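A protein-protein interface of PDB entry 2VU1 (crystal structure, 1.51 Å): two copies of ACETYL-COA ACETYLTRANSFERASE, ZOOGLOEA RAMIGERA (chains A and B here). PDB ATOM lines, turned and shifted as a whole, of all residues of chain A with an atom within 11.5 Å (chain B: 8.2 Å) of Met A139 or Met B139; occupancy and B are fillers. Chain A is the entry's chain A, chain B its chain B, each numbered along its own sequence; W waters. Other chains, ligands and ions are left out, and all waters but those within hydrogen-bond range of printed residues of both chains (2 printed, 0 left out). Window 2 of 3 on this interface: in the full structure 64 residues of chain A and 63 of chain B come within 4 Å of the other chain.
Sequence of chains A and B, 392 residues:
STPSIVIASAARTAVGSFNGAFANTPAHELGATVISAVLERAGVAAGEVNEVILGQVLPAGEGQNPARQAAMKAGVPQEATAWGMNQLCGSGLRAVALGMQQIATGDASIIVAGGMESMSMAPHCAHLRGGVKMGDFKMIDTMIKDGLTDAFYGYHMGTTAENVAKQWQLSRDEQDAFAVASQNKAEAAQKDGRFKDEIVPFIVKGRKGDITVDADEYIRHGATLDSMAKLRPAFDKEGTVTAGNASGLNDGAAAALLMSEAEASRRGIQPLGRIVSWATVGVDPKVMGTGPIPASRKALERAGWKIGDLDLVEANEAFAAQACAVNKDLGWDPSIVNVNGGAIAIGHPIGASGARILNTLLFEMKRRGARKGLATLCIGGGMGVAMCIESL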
ATOM      1  N   ALA A  60      16.982  16.779  23.222  1.00  0.00           N
ATOM      2  CA  ALA A  60      16.074  16.153  22.269  1.00  0.00           C
ATOM      3  C   ALA A  60      16.773  15.822  20.935  1.00  0.00           C
ATOM      4  O   ALA A  60      17.596  16.597  20.427  1.00  0.00           O
ATOM      5  CB  ALA A  60      14.851  16.979  22.054  1.00  0.00           C
ATOM      6  N   GLY A  61      16.630  14.568  20.556  1.00  0.00           N
ATOM      7  CA  GLY A  61      17.270  14.062  19.351  1.00  0.00           C
ATOM      8  C   GLY A  61      18.723  13.621  19.440  1.00  0.00           C
ATOM      9  O   GLY A  61      19.269  13.017  18.510  1.00  0.00           O
ATOM     10  N   GLU A  62      19.360  13.858  20.581  1.00  0.00           N
ATOM     11  CA  GLU A  62      20.775  13.551  20.740  1.00  0.00           C
ATOM     12  C   GLU A  62      21.023  12.064  21.100  1.00  0.00           C
ATOM     13  O   GLU A  62      22.151  11.585  21.077  1.00  0.00           O
ATOM     14  CB  GLU A  62      21.413  14.416  21.787  1.00  0.00           C
ATOM     15  CG  GLU A  62      22.910  14.251  21.788  1.00  0.00           C
ATOM     16  CD  GLU A  62      23.654  15.267  22.621  1.00  0.00           C
ATOM     17  OE1 GLU A  62      22.987  16.100  23.245  1.00  0.00           O
ATOM     18  OE2 GLU A  62      24.862  15.275  22.493  1.00  0.00           O
ATOM     19  N   MET A 121      21.841  22.917  18.122  1.00  0.00           N
ATOM     20  CA  MET A 121      21.424  21.606  17.609  1.00  0.00           C
ATOM     21  C   MET A 121      20.033  21.236  18.119  1.00  0.00           C
ATOM     22  O   MET A 121      19.541  20.181  17.828  1.00  0.00           O
ATOM     23  CB  MET A 121      22.476  20.511  17.992  1.00  0.00           C
ATOM     24  CG  MET A 121      23.711  20.496  17.135  1.00  0.00           C
ATOM     25  SD  MET A 121      23.407  20.018  15.482  1.00  0.00           S
ATOM     26  CE  MET A 121      23.346  18.211  15.625  1.00  0.00           C
ATOM     27  N   ALA A 122      19.416  22.067  18.949  1.00  0.00           N
ATOM     28  CA  ALA A 122      18.105  21.771  19.530  1.00  0.00           C
ATOM     29  C   ALA A 122      17.082  21.732  18.396  1.00  0.00           C
ATOM     30  O   ALA A 122      17.069  22.625  17.580  1.00  0.00           O
ATOM     31  CB  ALA A 122      17.756  22.817  20.617  1.00  0.00           C
ATOM     32  N   PRO A 123      16.252  20.680  18.284  1.00  0.00           N
ATOM     33  CA  PRO A 123      15.332  20.498  17.162  1.00  0.00           C
ATOM     34  C   PRO A 123      14.024  21.195  17.381  1.00  0.00           C
ATOM     35  O   PRO A 123      13.793  21.734  18.445  1.00  0.00           O
ATOM     36  CB  PRO A 123      15.096  18.969  17.111  1.00  0.00           C
ATOM     37  CG  PRO A 123      15.349  18.576  18.576  1.00  0.00           C
ATOM     38  CD  PRO A 123      16.310  19.534  19.191  1.00  0.00           C
ATOM     39  N   HIS A 124      13.248  21.201  16.339  1.00  0.00           N
ATOM     40  CA  HIS A 124      11.855  21.539  16.391  1.00  0.00           C
ATOM     41  C   HIS A 124      11.029  20.223  16.480  1.00  0.00           C
ATOM     42  O   HIS A 124      11.382  19.210  15.882  1.00  0.00           O
ATOM     43  CB  HIS A 124      11.410  22.270  15.124  1.00  0.00           C
ATOM     44  CG  HIS A 124      11.857  23.691  15.033  1.00  0.00           C
ATOM     45  ND1 HIS A 124      13.113  24.069  14.618  1.00  0.00           N
ATOM     46  CD2 HIS A 124      11.163  24.849  15.196  1.00  0.00           C
ATOM     47  CE1 HIS A 124      13.212  25.391  14.643  1.00  0.00           C
ATOM     48  NE2 HIS A 124      12.030  25.892  14.967  1.00  0.00           N
ATOM     49  N   CYS A 125       9.884  20.262  17.159  1.00  0.00           N
ATOM     50  CA  CYS A 125       9.141  19.038  17.451  1.00  0.00           C
ATOM     51  C   CYS A 125       7.668  19.228  17.399  1.00  0.00           C
ATOM     52  O   CYS A 125       7.156  20.353  17.413  1.00  0.00           O
ATOM     53  CB  CYS A 125       9.594  18.507  18.830  1.00  0.00           C
ATOM     54  SG  CYS A 125       8.976  19.423  20.236  1.00  0.00           S
ATOM     55  N   ALA A 126       6.966  18.102  17.212  1.00  0.00           N
ATOM     56  CA  ALA A 126       5.483  18.105  17.122  1.00  0.00           C
ATOM     57  C   ALA A 126       5.015  16.724  17.589  1.00  0.00           C
ATOM     58  O   ALA A 126       5.619  15.719  17.226  1.00  0.00           O
ATOM     59  CB  ALA A 126       5.014  18.368  15.723  1.00  0.00           C
ATOM     60  N   HIS A 127       4.019  16.692  18.476  1.00  0.00           N
ATOM     61  CA  HIS A 127       3.380  15.448  18.896  1.00  0.00           C
ATOM     62  C   HIS A 127       2.424  15.002  17.830  1.00  0.00           C
ATOM     63  O   HIS A 127       1.366  15.589  17.660  1.00  0.00           O
ATOM     64  CB  HIS A 127       2.611  15.666  20.204  1.00  0.00           C
ATOM     65  CG  HIS A 127       1.875  14.437  20.674  1.00  0.00           C
ATOM     66  ND1 HIS A 127       0.516  14.395  20.859  1.00  0.00           N
ATOM     67  CD2 HIS A 127       2.339  13.214  21.036  1.00  0.00           C
ATOM     68  CE1 HIS A 127       0.151  13.187  21.263  1.00  0.00           C
ATOM     69  NE2 HIS A 127       1.244  12.460  21.399  1.00  0.00           N
ATOM     70  N   LEU A 128       2.752  13.884  17.186  1.00  0.00           N
ATOM     71  CA  LEU A 128       2.071  13.444  15.978  1.00  0.00           C
ATOM     72  C   LEU A 128       1.430  12.068  16.028  1.00  0.00           C
ATOM     73  O   LEU A 128       0.829  11.643  14.966  1.00  0.00           O
ATOM     74  CB  LEU A 128       3.083  13.490  14.845  1.00  0.00           C
ATOM     75  CG  LEU A 128       3.460  14.931  14.492  1.00  0.00           C
ATOM     76  CD1 LEU A 128       4.681  15.049  13.638  1.00  0.00           C
ATOM     77  CD2 LEU A 128       2.323  15.500  13.759  1.00  0.00           C
ATOM     78  N   ARG A 129       1.402  11.453  17.210  1.00  0.00           N
ATOM     79  CA  ARG A 129       0.864  10.068  17.367  1.00  0.00           C
ATOM     80  C   ARG A 129      -0.610   9.919  17.110  1.00  0.00           C
ATOM     81  O   ARG A 129      -1.039   8.886  16.579  1.00  0.00           O
ATOM     82  CB  ARG A 129       1.173   9.488  18.756  1.00  0.00           C
ATOM     83  CG  ARG A 129       2.549   9.436  18.954  1.00  0.00           C
ATOM     84  CD  ARG A 129       3.003   8.553  20.143  1.00  0.00           C
ATOM     85  NE  ARG A 129       4.298   9.009  20.605  1.00  0.00           N
ATOM     86  CZ  ARG A 129       5.453   8.672  20.047  1.00  0.00           C
ATOM     87  NH1 ARG A 129       5.413   7.749  19.063  1.00  0.00           N
ATOM     88  NH2 ARG A 129       6.604   9.188  20.454  1.00  0.00           N
ATOM     89  N   VAL A 132      -2.925  14.289  12.637  1.00  0.00           N
ATOM     90  CA  VAL A 132      -3.505  15.621  12.503  1.00  0.00           C
ATOM     91  C   VAL A 132      -4.418  15.517  11.292  1.00  0.00           C
ATOM     92  O   VAL A 132      -3.999  15.751  10.158  1.00  0.00           O
ATOM     93  CB  VAL A 132      -2.435  16.738  12.316  1.00  0.00           C
ATOM     94  CG1 VAL A 132      -3.102  18.112  12.286  1.00  0.00           C
ATOM     95  CG2 VAL A 132      -1.336  16.664  13.424  1.00  0.00           C
ATOM     96  N   GLY A 135      -5.967  20.354   8.612  1.00  0.00           N
ATOM     97  CA  GLY A 135      -5.464  21.643   9.087  1.00  0.00           C
ATOM     98  C   GLY A 135      -3.969  21.687   9.394  1.00  0.00           C
ATOM     99  O   GLY A 135      -3.296  20.666   9.582  1.00  0.00           O
ATOM    100  N   ASP A 136      -3.461  22.904   9.482  1.00  0.00           N
ATOM    101  CA  ASP A 136      -2.056  23.133   9.782  1.00  0.00           C
ATOM    102  C   ASP A 136      -1.777  22.795  11.234  1.00  0.00           C
ATOM    103  O   ASP A 136      -2.688  22.788  12.053  1.00  0.00           O
ATOM    104  CB  ASP A 136      -1.678  24.600   9.553  1.00  0.00           C
ATOM    105  CG  ASP A 136      -2.017  25.083   8.163  1.00  0.00           C
ATOM    106  OD1 ASP A 136      -2.499  24.277   7.324  1.00  0.00           O
ATOM    107  OD2 ASP A 136      -1.823  26.287   7.909  1.00  0.00           O
ATOM    108  N   PHE A 137      -0.509  22.545  11.543  1.00  0.00           N
ATOM    109  CA  PHE A 137      -0.079  22.401  12.935  1.00  0.00           C
ATOM    110  C   PHE A 137       1.318  23.020  13.120  1.00  0.00           C
ATOM    111  O   PHE A 137       2.066  23.226  12.165  1.00  0.00           O
ATOM    112  CB  PHE A 137      -0.125  20.942  13.391  1.00  0.00           C
ATOM    113  CG  PHE A 137       0.829  20.059  12.684  1.00  0.00           C
ATOM    114  CD1 PHE A 137       2.138  19.917  13.158  1.00  0.00           C
ATOM    115  CD2 PHE A 137       0.440  19.354  11.576  1.00  0.00           C
ATOM    116  CE1 PHE A 137       3.032  19.094  12.500  1.00  0.00           C
ATOM    117  CE2 PHE A 137       1.326  18.544  10.907  1.00  0.00           C
ATOM    118  CZ  PHE A 137       2.637  18.424  11.363  1.00  0.00           C
ATOM    119  N   LYS A 138       1.621  23.327  14.356  1.00  0.00           N
ATOM    120  CA  LYS A 138       2.908  23.925  14.711  1.00  0.00           C
ATOM    121  C   LYS A 138       4.023  22.942  15.004  1.00  0.00           C
ATOM    122  O   LYS A 138       3.939  22.038  15.878  1.00  0.00           O
ATOM    123  CB  LYS A 138       2.766  24.886  15.906  1.00  0.00           C
ATOM    124  CG  LYS A 138       1.824  26.072  15.691  1.00  0.00           C
ATOM    125  CD  LYS A 138       1.812  26.949  16.959  1.00  0.00           C
ATOM    126  CE  LYS A 138       2.699  28.165  16.781  1.00  0.00           C
ATOM    127  NZ  LYS A 138       3.087  28.848  18.079  1.00  0.00           N
ATOM    128  N   MET A 139       5.147  23.250  14.388  1.00  0.00           N
ATOM    129  CA  MET A 139       6.409  22.688  14.761  1.00  0.00           C
ATOM    130  C   MET A 139       7.031  23.617  15.733  1.00  0.00           C
ATOM    131  O   MET A 139       7.349  24.744  15.384  1.00  0.00           O
ATOM    132  CB  MET A 139       7.273  22.543  13.504  1.00  0.00           C
ATOM    133  CG  MET A 139       6.755  21.337  12.653  1.00  0.00           C
ATOM    134  SD  MET A 139       7.199  19.758  13.335  1.00  0.00           S
ATOM    135  CE  MET A 139       9.028  19.731  13.266  1.00  0.00           C
ATOM    136  N   ILE A 140       7.211  23.094  16.946  1.00  0.00           N
ATOM    137  CA  ILE A 140       7.690  23.814  18.153  1.00  0.00           C
ATOM    138  C   ILE A 140       9.218  23.832  18.211  1.00  0.00           C
ATOM    139  O   ILE A 140       9.872  22.792  18.210  1.00  0.00           O
ATOM    140  CB  ILE A 140       7.105  23.141  19.380  1.00  0.00           C
ATOM    141  CG1 ILE A 140       5.587  23.196  19.311  1.00  0.00           C
ATOM    142  CG2 ILE A 140       7.567  23.749  20.641  1.00  0.00           C
ATOM    143  CD1 ILE A 140       5.083  24.563  19.133  1.00  0.00           C
ATOM    144  N   ASP A 141       9.780  25.022  18.400  1.00  0.00           N
ATOM    145  CA  ASP A 141      11.183  25.144  18.774  1.00  0.00           C
ATOM    146  C   ASP A 141      11.503  24.716  20.208  1.00  0.00           C
ATOM    147  O   ASP A 141      11.150  25.414  21.120  1.00  0.00           O
ATOM    148  CB  ASP A 141      11.658  26.618  18.548  1.00  0.00           C
ATOM    149  CG  ASP A 141      13.105  26.767  18.462  1.00  0.00           C
ATOM    150  OD1 ASP A 141      13.761  26.086  19.303  1.00  0.00           O
ATOM    151  OD2 ASP A 141      13.653  27.658  17.852  1.00  0.00           O
ATOM    152  N   THR A 142      12.114  23.558  20.377  1.00  0.00           N
ATOM    153  CA  THR A 142      12.408  22.986  21.707  1.00  0.00           C
ATOM    154  C   THR A 142      13.282  23.889  22.542  1.00  0.00           C
ATOM    155  O   THR A 142      13.084  24.020  23.722  1.00  0.00           O
ATOM    156  CB  THR A 142      12.955  21.533  21.668  1.00  0.00           C
ATOM    157  OG1 THR A 142      14.260  21.549  21.065  1.00  0.00           O
ATOM    158  CG2 THR A 142      11.950  20.553  20.936  1.00  0.00           C
ATOM    159  N   MET A 143      14.191  24.594  21.890  1.00  0.00           N
ATOM    160  CA  MET A 143      15.002  25.583  22.528  1.00  0.00           C
ATOM    161  C   MET A 143      14.151  26.648  23.193  1.00  0.00           C
ATOM    162  O   MET A 143      14.418  26.919  24.408  1.00  0.00           O
ATOM    163  CB  MET A 143      16.080  26.143  21.657  1.00  0.00           C
ATOM    164  CG  MET A 143      16.829  27.334  22.160  1.00  0.00           C
ATOM    165  SD  MET A 143      17.813  28.233  20.948  1.00  0.00           S
ATOM    166  CE  MET A 143      16.561  29.110  20.116  1.00  0.00           C
ATOM    167  N   ILE A 144      13.203  27.235  22.478  1.00  0.00           N
ATOM    168  CA  ILE A 144      12.355  28.280  23.100  1.00  0.00           C
ATOM    169  C   ILE A 144      11.378  27.687  24.150  1.00  0.00           C
ATOM    170  O   ILE A 144      11.326  28.127  25.312  1.00  0.00           O
ATOM    171  CB  ILE A 144      11.672  29.035  22.037  1.00  0.00           C
ATOM    172  CG1 ILE A 144      12.744  29.734  21.143  1.00  0.00           C
ATOM    173  CG2 ILE A 144      10.695  30.012  22.664  1.00  0.00           C
ATOM    174  CD1 ILE A 144      12.181  30.339  19.931  1.00  0.00           C
ATOM    175  N   LYS A 145      10.768  26.598  23.793  1.00  0.00           N
ATOM    176  CA  LYS A 145       9.761  25.983  24.591  1.00  0.00           C
ATOM    177  C   LYS A 145      10.331  25.440  25.874  1.00  0.00           C
ATOM    178  O   LYS A 145       9.803  25.708  26.933  1.00  0.00           O
ATOM    179  CB  LYS A 145       9.026  24.886  23.745  1.00  0.00           C
ATOM    180  CG  LYS A 145       8.002  24.111  24.582  1.00  0.00           C
ATOM    181  CD  LYS A 145       6.856  24.962  24.891  1.00  0.00           C
ATOM    182  CE  LYS A 145       5.732  24.130  25.515  1.00  0.00           C
ATOM    183  NZ  LYS A 145       4.600  25.004  25.662  1.00  0.00           N
ATOM    184  N   ASP A 146      11.371  24.645  25.770  1.00  0.00           N
ATOM    185  CA  ASP A 146      11.908  23.921  26.910  1.00  0.00           C
ATOM    186  C   ASP A 146      12.963  24.699  27.606  1.00  0.00           C
ATOM    187  O   ASP A 146      13.236  24.428  28.801  1.00  0.00           O
ATOM    188  CB  ASP A 146      12.363  22.501  26.420  1.00  0.00           C
ATOM    189  CG  ASP A 146      11.207  21.671  25.741  1.00  0.00           C
ATOM    190  OD1 ASP A 146       9.960  21.827  25.935  1.00  0.00           O
ATOM    191  OD2 ASP A 146      11.517  20.765  24.945  1.00  0.00           O
ATOM    192  N   PRO B 123       7.267  13.687  21.360  1.00  0.00           N
ATOM    193  CA  PRO B 123       7.092  14.173  20.004  1.00  0.00           C
ATOM    194  C   PRO B 123       8.085  13.600  19.013  1.00  0.00           C
ATOM    195  O   PRO B 123       9.026  12.949  19.400  1.00  0.00           O
ATOM    196  CB  PRO B 123       7.302  15.702  20.100  1.00  0.00           C
ATOM    197  CG  PRO B 123       8.283  15.782  21.215  1.00  0.00           C
ATOM    198  CD  PRO B 123       8.017  14.653  22.179  1.00  0.00           C
ATOM    199  N   HIS B 124       7.855  13.927  17.761  1.00  0.00           N
ATOM    200  CA  HIS B 124       8.826  13.688  16.749  1.00  0.00           C
ATOM    201  C   HIS B 124       9.582  15.001  16.549  1.00  0.00           C
ATOM    202  O   HIS B 124       8.954  16.096  16.561  1.00  0.00           O
ATOM    203  CB  HIS B 124       8.092  13.324  15.401  1.00  0.00           C
ATOM    204  CG  HIS B 124       7.597  11.901  15.356  1.00  0.00           C
ATOM    205  ND1 HIS B 124       6.470  11.464  16.020  1.00  0.00           N
ATOM    206  CD2 HIS B 124       8.110  10.810  14.726  1.00  0.00           C
ATOM    207  CE1 HIS B 124       6.357  10.145  15.873  1.00  0.00           C
ATOM    208  NE2 HIS B 124       7.333   9.733  15.079  1.00  0.00           N
ATOM    209  N   CYS B 125      10.839  14.905  16.105  1.00  0.00           N
ATOM    210  CA  CYS B 125      11.646  16.097  15.956  1.00  0.00           C
ATOM    211  C   CYS B 125      12.623  16.085  14.812  1.00  0.00           C
ATOM    212  O   CYS B 125      13.016  15.033  14.306  1.00  0.00           O
ATOM    213  CB  CYS B 125      12.428  16.321  17.267  1.00  0.00           C
ATOM    214  SG  CYS B 125      13.800  15.235  17.567  1.00  0.00           S
ATOM    215  N   ALA B 126      13.071  17.278  14.461  1.00  0.00           N
ATOM    216  CA  ALA B 126      14.145  17.389  13.521  1.00  0.00           C
ATOM    217  C   ALA B 126      14.848  18.706  13.722  1.00  0.00           C
ATOM    218  O   ALA B 126      14.262  19.691  14.090  1.00  0.00           O
ATOM    219  CB  ALA B 126      13.642  17.264  12.145  1.00  0.00           C
ATOM    220  N   HIS B 127      16.157  18.672  13.578  1.00  0.00           N
ATOM    221  CA  HIS B 127      16.999  19.830  13.644  1.00  0.00           C
ATOM    222  C   HIS B 127      16.882  20.524  12.296  1.00  0.00           C
ATOM    223  O   HIS B 127      17.399  20.032  11.296  1.00  0.00           O
ATOM    224  CB  HIS B 127      18.456  19.403  13.930  1.00  0.00           C
ATOM    225  CG  HIS B 127      19.405  20.556  13.935  1.00  0.00           C
ATOM    226  ND1 HIS B 127      20.475  20.645  13.074  1.00  0.00           N
ATOM    227  CD2 HIS B 127      19.383  21.714  14.640  1.00  0.00           C
ATOM    228  CE1 HIS B 127      21.093  21.796  13.265  1.00  0.00           C
ATOM    229  NE2 HIS B 127      20.464  22.451  14.229  1.00  0.00           N
ATOM    230  N   LEU B 128      16.300  21.732  12.274  1.00  0.00           N
ATOM    231  CA  LEU B 128      16.023  22.452  11.063  1.00  0.00           C
ATOM    232  C   LEU B 128      16.585  23.843  10.983  1.00  0.00           C
ATOM    233  O   LEU B 128      16.169  24.597  10.094  1.00  0.00           O
ATOM    234  CB  LEU B 128      14.496  22.533  10.915  1.00  0.00           C
ATOM    235  CG  LEU B 128      13.834  21.162  10.749  1.00  0.00           C
ATOM    236  CD1 LEU B 128      12.384  21.249  11.170  1.00  0.00           C
ATOM    237  CD2 LEU B 128      14.055  20.650   9.310  1.00  0.00           C
ATOM    238  N   ASP B 136      15.585  14.521   1.165  1.00  0.00           N
ATOM    239  CA  ASP B 136      14.711  14.126   2.260  1.00  0.00           C
ATOM    240  C   ASP B 136      15.409  14.183   3.594  1.00  0.00           C
ATOM    241  O   ASP B 136      16.646  14.146   3.682  1.00  0.00           O
ATOM    242  CB  ASP B 136      14.219  12.691   2.072  1.00  0.00           C
ATOM    243  CG  ASP B 136      13.575  12.444   0.716  1.00  0.00           C
ATOM    244  OD1 ASP B 136      13.267  13.427   0.005  1.00  0.00           O
ATOM    245  OD2 ASP B 136      13.375  11.241   0.380  1.00  0.00           O
ATOM    246  N   PHE B 137      14.608  14.255   4.649  1.00  0.00           N
ATOM    247  CA  PHE B 137      15.140  14.222   5.993  1.00  0.00           C
ATOM    248  C   PHE B 137      14.155  13.490   6.896  1.00  0.00           C
ATOM    249  O   PHE B 137      12.973  13.418   6.617  1.00  0.00           O
ATOM    250  CB  PHE B 137      15.495  15.619   6.517  1.00  0.00           C
ATOM    251  CG  PHE B 137      14.314  16.511   6.811  1.00  0.00           C
ATOM    252  CD1 PHE B 137      13.858  17.432   5.891  1.00  0.00           C
ATOM    253  CD2 PHE B 137      13.736  16.499   8.061  1.00  0.00           C
ATOM    254  CE1 PHE B 137      12.790  18.293   6.202  1.00  0.00           C
ATOM    255  CE2 PHE B 137      12.679  17.341   8.379  1.00  0.00           C
ATOM    256  CZ  PHE B 137      12.206  18.236   7.481  1.00  0.00           C
ATOM    257  N   LYS B 138      14.674  12.949   7.986  1.00  0.00           N
ATOM    258  CA  LYS B 138      13.843  12.240   8.929  1.00  0.00           C
ATOM    259  C   LYS B 138      13.266  13.134  10.029  1.00  0.00           C
ATOM    260  O   LYS B 138      13.959  13.967  10.657  1.00  0.00           O
ATOM    261  CB  LYS B 138      14.647  11.114   9.527  1.00  0.00           C
ATOM    262  CG  LYS B 138      15.000  10.087   8.521  1.00  0.00           C
ATOM    263  CD  LYS B 138      15.688   8.954   9.202  1.00  0.00           C
ATOM    264  CE  LYS B 138      15.478   7.660   8.485  1.00  0.00           C
ATOM    265  NZ  LYS B 138      16.634   7.372   7.587  1.00  0.00           N
ATOM    266  N   MET B 139      11.984  12.934  10.286  1.00  0.00           N
ATOM    267  CA  MET B 139      11.394  13.354  11.544  1.00  0.00           C
ATOM    268  C   MET B 139      11.535  12.184  12.506  1.00  0.00           C
ATOM    269  O   MET B 139      10.976  11.080  12.306  1.00  0.00           O
ATOM    270  CB  MET B 139       9.940  13.742  11.369  1.00  0.00           C
ATOM    271  CG  MET B 139       9.730  15.164  10.760  1.00  0.00           C
ATOM    272  SD  MET B 139      10.029  16.383  12.015  1.00  0.00           S
ATOM    273  CE  MET B 139       8.608  16.243  13.122  1.00  0.00           C
ATOM    274  N   ILE B 140      12.303  12.410  13.567  1.00  0.00           N
ATOM    275  CA  ILE B 140      12.788  11.384  14.455  1.00  0.00           C
ATOM    276  C   ILE B 140      11.786  11.216  15.567  1.00  0.00           C
ATOM    277  O   ILE B 140      11.370  12.152  16.194  1.00  0.00           O
ATOM    278  CB  ILE B 140      14.105  11.851  15.037  1.00  0.00           C
ATOM    279  CG1 ILE B 140      15.099  12.094  13.893  1.00  0.00           C
ATOM    280  CG2 ILE B 140      14.588  10.920  16.091  1.00  0.00           C
ATOM    281  CD1 ILE B 140      15.144  11.053  12.878  1.00  0.00           C
ATOM    282  N   ASP B 141      11.409   9.984  15.855  1.00  0.00           N
ATOM    283  CA  ASP B 141      10.677   9.716  17.080  1.00  0.00           C
ATOM    284  C   ASP B 141      11.525   9.796  18.326  1.00  0.00           C
ATOM    285  O   ASP B 141      12.312   8.938  18.595  1.00  0.00           O
ATOM    286  CB  ASP B 141      10.004   8.340  16.923  1.00  0.00           C
ATOM    287  CG  ASP B 141       9.021   8.046  17.983  1.00  0.00           C
ATOM    288  OD1 ASP B 141       9.293   8.458  19.155  1.00  0.00           O
ATOM    289  OD2 ASP B 141       8.088   7.268  17.744  1.00  0.00           O
ATOM    290  N   THR B 142      11.354  10.879  19.082  1.00  0.00           N
ATOM    291  CA  THR B 142      12.136  11.048  20.290  1.00  0.00           C
ATOM    292  C   THR B 142      12.077   9.921  21.314  1.00  0.00           C
ATOM    293  O   THR B 142      13.039   9.647  21.989  1.00  0.00           O
ATOM    294  CB  THR B 142      11.845  12.430  20.993  1.00  0.00           C
ATOM    295  OG1 THR B 142      10.525  12.457  21.595  1.00  0.00           O
ATOM    296  CG2 THR B 142      12.073  13.575  20.045  1.00  0.00           C
HETATM  297  O   HOH W   1      15.853  22.948  14.887  1.00  0.00           O
HETATM  298  O   HOH W   2       4.769  12.171  18.142  1.00  0.00           O
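Water W2 lies within hydrogen-bond range of ND1 of His B124 (2.8 Å) and N of Leu A128 (2.8 Å).
Water W1 lies within hydrogen-bond range of N of Leu B128 (2.9 Å), ND1 of His A124 (3.0 Å) and O of Ala A122 (3.0 Å).
Of chain B, only Met B139 comes within 4 Å of Met A139.
Met B139 touches just one residue of chain A: Met A139.
Ala B126 touches just these residues of chain A: Pro A123 (3.2 Å) and His A124 (2.9 Å).
No residue of chain A comes within 4 Å of Ile B140.
Printed residues of chain B within 4 Å of His A124: Cys B125 (3.1 Å) and Ala B126 (2.9 Å).
Of the printed residues of chain B, Pro A123 touches Cys B125 (3.8 Å), Ala B126 (3.2 Å) and His B127 (3.7 Å).
Lys A145 touches none of the printed residues of chain B.
The nearest residue of chain B that does not touch Met A139 is Leu B128 (4.2 Å).
The nearest printed residue of chain A that does not touch Asp B141 is Gly A61 (7.2 Å).
Printed residues of chain B that touch a printed residue of chain A: Pro B123, His B124, Cys B125, Ala B126, His B127, Met B139 and Asp B141.
Hydrophobic or aromatic side chains of chain A that line the printed part of chain B: Met A121, Pro A123, His A124 and Met A139.
The backbone NH of His A124 sits at hydrogen-bond distance from the backbone carbonyl oxygen of Ala B126.
N of Ala A126 sits at hydrogen-bond distance from O of His B124 (2.9 Å).
The guanidinium group of Arg A129 is in salt-bridge range of the side-chain carboxylate of Asp B141.
Pro A123 touches Ala B126, and with the chains exchanged Ala A126 touches Pro B123.
Pro A123 touches His B127, and with the chains exchanged His A127 touches Pro B123.
Cys A125 touches its own counterpart, Cys B125.
Met A139 touches its own counterpart, Met B139.
13 positions are printed for both chains.
Among the printed residues, merely in contact across the chains: Met A121 with His B127, Ala A122 with His B127, Pro A123 with Cys B125, Pro A123 with Ala B126, Pro A123 with His B127, His A124 with Cys B125, Cys A125 with Pro B123, Cys A125 with His B124, Cys A125 with Cys B125, Ala A126 with Pro B123, His A127 with Pro B123 and Met A139 with Met B139.
The backbone NH (N) of Cys A125 is in hydrogen-bond range of the backbone carbonyl oxygen (O) of Ile A140, at 2.7 Å.
The backbone NH (N) of Cys B125 lies within hydrogen-bond range of the backbone carbonyl oxygen (O) of Ile B140.
The backbone carbonyl oxygen (O) of Pro B123 is in hydrogen-bond range of the side-chain hydroxyl (OG1) of Thr B142, at 2.7 Å.
OG1 of Thr A142 lies within hydrogen-bond range of O of Pro A123, 2.7 Å away.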
